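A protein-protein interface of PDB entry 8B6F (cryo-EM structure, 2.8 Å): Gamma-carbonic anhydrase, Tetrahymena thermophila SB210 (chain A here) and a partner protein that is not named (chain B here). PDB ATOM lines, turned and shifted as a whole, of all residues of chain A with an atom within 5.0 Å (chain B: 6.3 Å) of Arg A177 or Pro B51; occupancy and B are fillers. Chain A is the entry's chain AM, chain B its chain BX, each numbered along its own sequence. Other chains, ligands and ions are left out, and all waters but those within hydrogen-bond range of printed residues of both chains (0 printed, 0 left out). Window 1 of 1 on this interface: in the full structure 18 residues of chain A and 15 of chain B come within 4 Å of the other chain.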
ATOM      1  N   GLY A 158       7.668  -4.747  30.565  1.00  0.00           N
ATOM      2  CA  GLY A 158       7.176  -3.564  29.889  1.00  0.00           C
ATOM      3  C   GLY A 158       5.845  -3.049  30.375  1.00  0.00           C
ATOM      4  O   GLY A 158       5.251  -2.194  29.714  1.00  0.00           O
ATOM      5  N   SER A 159       5.361  -3.534  31.509  1.00  0.00           N
ATOM      6  CA  SER A 159       4.080  -3.114  32.056  1.00  0.00           C
ATOM      7  C   SER A 159       4.282  -1.906  32.959  1.00  0.00           C
ATOM      8  O   SER A 159       5.167  -1.908  33.820  1.00  0.00           O
ATOM      9  CB  SER A 159       3.422  -4.270  32.802  1.00  0.00           C
ATOM     10  OG  SER A 159       4.291  -4.785  33.783  1.00  0.00           O
ATOM     11  N   VAL A 160       3.463  -0.879  32.757  1.00  0.00           N
ATOM     12  CA  VAL A 160       3.568   0.382  33.480  1.00  0.00           C
ATOM     13  C   VAL A 160       2.281   0.608  34.254  1.00  0.00           C
ATOM     14  O   VAL A 160       1.187   0.566  33.680  1.00  0.00           O
ATOM     15  CB  VAL A 160       3.840   1.555  32.520  1.00  0.00           C
ATOM     16  CG1 VAL A 160       3.841   2.881  33.267  1.00  0.00           C
ATOM     17  CG2 VAL A 160       5.158   1.346  31.796  1.00  0.00           C
ATOM     18  N   VAL A 173      -1.006  -8.924  35.027  1.00  0.00           N
ATOM     19  CA  VAL A 173      -0.876  -7.790  34.117  1.00  0.00           C
ATOM     20  C   VAL A 173      -0.081  -8.268  32.904  1.00  0.00           C
ATOM     21  O   VAL A 173       1.110  -8.587  33.048  1.00  0.00           O
ATOM     22  CB  VAL A 173      -0.188  -6.599  34.795  1.00  0.00           C
ATOM     23  CG1 VAL A 173      -0.039  -5.440  33.820  1.00  0.00           C
ATOM     24  CG2 VAL A 173      -0.964  -6.164  36.023  1.00  0.00           C
ATOM     25  N   PRO A 174      -0.680  -8.342  31.716  1.00  0.00           N
ATOM     26  CA  PRO A 174       0.076  -8.809  30.549  1.00  0.00           C
ATOM     27  C   PRO A 174       1.241  -7.885  30.236  1.00  0.00           C
ATOM     28  O   PRO A 174       1.212  -6.688  30.524  1.00  0.00           O
ATOM     29  CB  PRO A 174      -0.964  -8.801  29.422  1.00  0.00           C
ATOM     30  CG  PRO A 174      -2.279  -8.835  30.107  1.00  0.00           C
ATOM     31  CD  PRO A 174      -2.093  -8.092  31.387  1.00  0.00           C
ATOM     32  N   ALA A 175       2.280  -8.462  29.642  1.00  0.00           N
ATOM     33  CA  ALA A 175       3.485  -7.703  29.345  1.00  0.00           C
ATOM     34  C   ALA A 175       3.176  -6.544  28.406  1.00  0.00           C
ATOM     35  O   ALA A 175       2.333  -6.650  27.512  1.00  0.00           O
ATOM     36  CB  ALA A 175       4.539  -8.615  28.718  1.00  0.00           C
ATOM     37  N   GLY A 176       3.861  -5.424  28.623  1.00  0.00           N
ATOM     38  CA  GLY A 176       3.733  -4.277  27.747  1.00  0.00           C
ATOM     39  C   GLY A 176       2.362  -3.636  27.740  1.00  0.00           C
ATOM     40  O   GLY A 176       1.833  -3.323  26.669  1.00  0.00           O
ATOM     41  N   ARG A 177       1.771  -3.430  28.914  1.00  0.00           N
ATOM     42  CA  ARG A 177       0.457  -2.812  29.009  1.00  0.00           C
ATOM     43  C   ARG A 177       0.457  -1.773  30.120  1.00  0.00           C
ATOM     44  O   ARG A 177       1.314  -1.775  31.005  1.00  0.00           O
ATOM     45  CB  ARG A 177      -0.640  -3.855  29.246  1.00  0.00           C
ATOM     46  CG  ARG A 177      -0.805  -4.813  28.081  1.00  0.00           C
ATOM     47  CD  ARG A 177      -2.100  -5.588  28.168  1.00  0.00           C
ATOM     48  NE  ARG A 177      -2.252  -6.502  27.042  1.00  0.00           N
ATOM     49  CZ  ARG A 177      -2.782  -6.174  25.872  1.00  0.00           C
ATOM     50  NH1 ARG A 177      -3.230  -4.953  25.632  1.00  0.00           N
ATOM     51  NH2 ARG A 177      -2.866  -7.094  24.918  1.00  0.00           N
ATOM     52  N   LEU A 178      -0.524  -0.879  30.052  1.00  0.00           N
ATOM     53  CA  LEU A 178      -0.625   0.273  30.935  1.00  0.00           C
ATOM     54  C   LEU A 178      -1.834   0.134  31.848  1.00  0.00           C
ATOM     55  O   LEU A 178      -2.922  -0.245  31.404  1.00  0.00           O
ATOM     56  CB  LEU A 178      -0.737   1.567  30.123  1.00  0.00           C
ATOM     57  CG  LEU A 178      -0.936   2.867  30.905  1.00  0.00           C
ATOM     58  CD1 LEU A 178       0.287   3.179  31.745  1.00  0.00           C
ATOM     59  CD2 LEU A 178      -1.243   4.013  29.962  1.00  0.00           C
ATOM     60  N   ILE A 179      -1.635   0.447  33.124  1.00  0.00           N
ATOM     61  CA  ILE A 179      -2.718   0.513  34.100  1.00  0.00           C
ATOM     62  C   ILE A 179      -2.845   1.970  34.529  1.00  0.00           C
ATOM     63  O   ILE A 179      -2.059   2.435  35.366  1.00  0.00           O
ATOM     64  CB  ILE A 179      -2.454  -0.412  35.299  1.00  0.00           C
ATOM     65  CG1 ILE A 179      -2.196  -1.847  34.830  1.00  0.00           C
ATOM     66  CG2 ILE A 179      -3.623  -0.371  36.270  1.00  0.00           C
ATOM     67  CD1 ILE A 179      -3.322  -2.457  34.017  1.00  0.00           C
ATOM     68  N   PRO A 180      -3.804   2.724  33.994  1.00  0.00           N
ATOM     69  CA  PRO A 180      -3.867   4.161  34.290  1.00  0.00           C
ATOM     70  C   PRO A 180      -4.036   4.433  35.777  1.00  0.00           C
ATOM     71  O   PRO A 180      -4.251   3.538  36.596  1.00  0.00           O
ATOM     72  CB  PRO A 180      -5.083   4.638  33.491  1.00  0.00           C
ATOM     73  CG  PRO A 180      -5.231   3.644  32.402  1.00  0.00           C
ATOM     74  CD  PRO A 180      -4.801   2.333  32.982  1.00  0.00           C
ATOM     75  N   TRP A 185      -8.204  -2.674  38.641  1.00  0.00           N
ATOM     76  CA  TRP A 185      -8.177  -3.693  37.600  1.00  0.00           C
ATOM     77  C   TRP A 185      -8.059  -5.068  38.240  1.00  0.00           C
ATOM     78  O   TRP A 185      -7.290  -5.255  39.186  1.00  0.00           O
ATOM     79  CB  TRP A 185      -7.015  -3.454  36.631  1.00  0.00           C
ATOM     80  CG  TRP A 185      -7.182  -2.219  35.798  1.00  0.00           C
ATOM     81  CD1 TRP A 185      -7.127  -0.926  36.230  1.00  0.00           C
ATOM     82  CD2 TRP A 185      -7.429  -2.159  34.388  1.00  0.00           C
ATOM     83  NE1 TRP A 185      -7.325  -0.066  35.178  1.00  0.00           N
ATOM     84  CE2 TRP A 185      -7.515  -0.799  34.036  1.00  0.00           C
ATOM     85  CE3 TRP A 185      -7.590  -3.125  33.390  1.00  0.00           C
ATOM     86  CZ2 TRP A 185      -7.751  -0.379  32.730  1.00  0.00           C
ATOM     87  CZ3 TRP A 185      -7.825  -2.706  32.093  1.00  0.00           C
ATOM     88  CH2 TRP A 185      -7.904  -1.346  31.774  1.00  0.00           C
ATOM     89  N   ALA B  39      -2.718   6.134  23.867  1.00  0.00           N
ATOM     90  CA  ALA B  39      -3.229   5.101  24.756  1.00  0.00           C
ATOM     91  C   ALA B  39      -4.514   5.575  25.422  1.00  0.00           C
ATOM     92  O   ALA B  39      -4.570   6.685  25.961  1.00  0.00           O
ATOM     93  CB  ALA B  39      -2.187   4.742  25.816  1.00  0.00           C
ATOM     94  N   LYS B  40      -5.545   4.736  25.373  1.00  0.00           N
ATOM     95  CA  LYS B  40      -6.801   5.047  26.040  1.00  0.00           C
ATOM     96  C   LYS B  40      -6.603   5.053  27.552  1.00  0.00           C
ATOM     97  O   LYS B  40      -5.890   4.210  28.102  1.00  0.00           O
ATOM     98  CB  LYS B  40      -7.869   4.029  25.646  1.00  0.00           C
ATOM     99  CG  LYS B  40      -9.245   4.285  26.243  1.00  0.00           C
ATOM    100  CD  LYS B  40     -10.234   3.224  25.789  1.00  0.00           C
ATOM    101  CE  LYS B  40     -11.606   3.442  26.401  1.00  0.00           C
ATOM    102  NZ  LYS B  40     -12.587   2.416  25.947  1.00  0.00           N
ATOM    103  N   ARG B  41      -7.235   6.020  28.226  1.00  0.00           N
ATOM    104  CA  ARG B  41      -7.074   6.152  29.669  1.00  0.00           C
ATOM    105  C   ARG B  41      -8.388   6.443  30.388  1.00  0.00           C
ATOM    106  O   ARG B  41      -8.365   6.854  31.555  1.00  0.00           O
ATOM    107  CB  ARG B  41      -6.063   7.255  30.001  1.00  0.00           C
ATOM    108  CG  ARG B  41      -4.631   6.898  29.649  1.00  0.00           C
ATOM    109  CD  ARG B  41      -3.666   7.950  30.163  1.00  0.00           C
ATOM    110  NE  ARG B  41      -2.275   7.555  29.971  1.00  0.00           N
ATOM    111  CZ  ARG B  41      -1.574   7.770  28.867  1.00  0.00           C
ATOM    112  NH1 ARG B  41      -2.104   8.375  27.816  1.00  0.00           N
ATOM    113  NH2 ARG B  41      -0.308   7.368  28.815  1.00  0.00           N
ATOM    114  N   PHE B  44     -13.314   2.861  29.833  1.00  0.00           N
ATOM    115  CA  PHE B  44     -13.117   1.447  29.566  1.00  0.00           C
ATOM    116  C   PHE B  44     -14.401   0.667  29.834  1.00  0.00           C
ATOM    117  O   PHE B  44     -15.347   1.155  30.458  1.00  0.00           O
ATOM    118  CB  PHE B  44     -11.985   0.890  30.429  1.00  0.00           C
ATOM    119  CG  PHE B  44     -10.637   1.460  30.107  1.00  0.00           C
ATOM    120  CD1 PHE B  44      -9.837   0.871  29.141  1.00  0.00           C
ATOM    121  CD2 PHE B  44     -10.162   2.573  30.775  1.00  0.00           C
ATOM    122  CE1 PHE B  44      -8.593   1.387  28.845  1.00  0.00           C
ATOM    123  CE2 PHE B  44      -8.918   3.094  30.483  1.00  0.00           C
ATOM    124  CZ  PHE B  44      -8.133   2.500  29.515  1.00  0.00           C
ATOM    125  N   GLN B  49      -9.471  -5.077  26.735  1.00  0.00           N
ATOM    126  CA  GLN B  49      -8.129  -5.344  27.225  1.00  0.00           C
ATOM    127  C   GLN B  49      -7.458  -4.051  27.679  1.00  0.00           C
ATOM    128  O   GLN B  49      -7.859  -2.945  27.308  1.00  0.00           O
ATOM    129  CB  GLN B  49      -7.286  -6.016  26.141  1.00  0.00           C
ATOM    130  CG  GLN B  49      -7.859  -7.329  25.638  1.00  0.00           C
ATOM    131  CD  GLN B  49      -7.016  -7.947  24.544  1.00  0.00           C
ATOM    132  OE1 GLN B  49      -6.039  -7.355  24.089  1.00  0.00           O
ATOM    133  NE2 GLN B  49      -7.388  -9.148  24.117  1.00  0.00           N
ATOM    134  N   ALA B  50      -6.423  -4.204  28.497  1.00  0.00           N
ATOM    135  CA  ALA B  50      -5.696  -3.049  28.990  1.00  0.00           C
ATOM    136  C   ALA B  50      -4.914  -2.388  27.855  1.00  0.00           C
ATOM    137  O   ALA B  50      -4.471  -3.061  26.920  1.00  0.00           O
ATOM    138  CB  ALA B  50      -4.742  -3.456  30.108  1.00  0.00           C
ATOM    139  N   PRO B  51      -4.727  -1.067  27.912  1.00  0.00           N
ATOM    140  CA  PRO B  51      -3.983  -0.384  26.844  1.00  0.00           C
ATOM    141  C   PRO B  51      -2.497  -0.696  26.882  1.00  0.00           C
ATOM    142  O   PRO B  51      -2.032  -1.424  27.763  1.00  0.00           O
ATOM    143  CB  PRO B  51      -4.257   1.099  27.123  1.00  0.00           C
ATOM    144  CG  PRO B  51      -4.511   1.159  28.582  1.00  0.00           C
ATOM    145  CD  PRO B  51      -5.196  -0.126  28.945  1.00  0.00           C
ATOM    146  N   PHE B  52      -1.746  -0.156  25.928  1.00  0.00           N
ATOM    147  CA  PHE B  52      -0.311  -0.376  25.840  1.00  0.00           C
ATOM    148  C   PHE B  52       0.449   0.807  26.430  1.00  0.00           C
ATOM    149  O   PHE B  52      -0.001   1.953  26.370  1.00  0.00           O
ATOM    150  CB  PHE B  52       0.115  -0.603  24.389  1.00  0.00           C
ATOM    151  CG  PHE B  52      -0.457  -1.850  23.786  1.00  0.00           C
ATOM    152  CD1 PHE B  52       0.136  -3.079  24.014  1.00  0.00           C
ATOM    153  CD2 PHE B  52      -1.590  -1.794  22.994  1.00  0.00           C
ATOM    154  CE1 PHE B  52      -0.389  -4.228  23.464  1.00  0.00           C
ATOM    155  CE2 PHE B  52      -2.121  -2.941  22.439  1.00  0.00           C
ATOM    156  CZ  PHE B  52      -1.519  -4.159  22.675  1.00  0.00           C
ATOM    157  N   ALA B  53       1.615   0.512  27.005  1.00  0.00           N
ATOM    158  CA  ALA B  53       2.370   1.529  27.726  1.00  0.00           C
ATOM    159  C   ALA B  53       3.245   2.362  26.796  1.00  0.00           C
ATOM    160  O   ALA B  53       3.369   3.577  26.983  1.00  0.00           O
ATOM    161  CB  ALA B  53       3.228   0.873  28.807  1.00  0.00           C
ATOM    162  N   TYR B  54       3.857   1.733  25.797  1.00  0.00           N
ATOM    163  CA  TYR B  54       4.783   2.400  24.890  1.00  0.00           C
ATOM    164  C   TYR B  54       4.140   2.501  23.515  1.00  0.00           C
ATOM    165  O   TYR B  54       3.781   1.481  22.919  1.00  0.00           O
ATOM    166  CB  TYR B  54       6.109   1.643  24.819  1.00  0.00           C
ATOM    167  CG  TYR B  54       6.729   1.403  26.176  1.00  0.00           C
ATOM    168  CD1 TYR B  54       6.399   0.279  26.922  1.00  0.00           C
ATOM    169  CD2 TYR B  54       7.634   2.307  26.716  1.00  0.00           C
ATOM    170  CE1 TYR B  54       6.959   0.058  28.164  1.00  0.00           C
ATOM    171  CE2 TYR B  54       8.199   2.094  27.957  1.00  0.00           C
ATOM    172  CZ  TYR B  54       7.856   0.970  28.676  1.00  0.00           C
ATOM    173  OH  TYR B  54       8.414   0.753  29.912  1.00  0.00           O
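Hydrophobic or aromatic side chains of chain B within 4 Å of the printed part of chain A: Phe B44, Ala B50, Pro B51, Phe B52, Ala B53 and Tyr B54.
Among the printed residues, 18 pairs touch across the chains.
The backbone carbonyl oxygen (O) of Arg A177 sits at hydrogen-bond distance from the backbone NH (N) of Val A160.
O of Val A160 sits at hydrogen-bond distance from N of Ile A179, at 2.9 Å.
The side-chain amide oxygen of Gln B49 sits at hydrogen-bond distance from the guanidinium group of Arg A177 (3.3 Å).
NH1 of Arg A177 sits at hydrogen-bond distance from O of Ala B50, 2.6 Å away.
The backbone NH of Leu A178 is in hydrogen-bond range of the backbone carbonyl oxygen of Pro B51, 2.8 Å away.
Of the printed residues of chain B, Gly A176 touches Phe B52 and Ala B53.
Arg A177 touches five residues of chain B.
Printed residues of chain B within 4 Å of Trp A185: Phe B44 and Ala B50.
Of the printed residues of chain A, Gln B49 touches Arg A177 (3.3 Å).
Of the printed residues of chain A, Pro B51 touches Arg A177 (3.1 Å) and Leu A178 (2.8 Å).
Printed residues of chain A within 4 Å of Phe B52: Gly A176, Arg A177 and Leu A178.
The nearest printed residue of chain B that does not touch Arg A177 is Tyr B54 (6.3 Å).
Among the printed residues, pairs that only touch across the chains: Gly A158 with Ala B53 (3.8 Å), Gly A158 with Tyr B54 (3.2 Å), Val A160 with Ala B53 (3.6 Å), Val A160 with Tyr B54 (3.8 Å), Gly A176 with Phe B52 (3.2 Å), Gly A176 with Ala B53 (3.9 Å), Arg A177 with Pro B51 (3.1 Å), Arg A177 with Phe B52 (3.5 Å), Arg A177 with Ala B53 (3.9 Å), Leu A178 with Arg B41 (3.7 Å), Leu A178 with Ala B50 (3.9 Å), Leu A178 with Phe B52 (3.8 Å), Leu A178 with Ala B53 (3.9 Å), Trp A185 with Phe B44 (3.9 Å) and Trp A185 with Ala B50 (3.7 Å).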
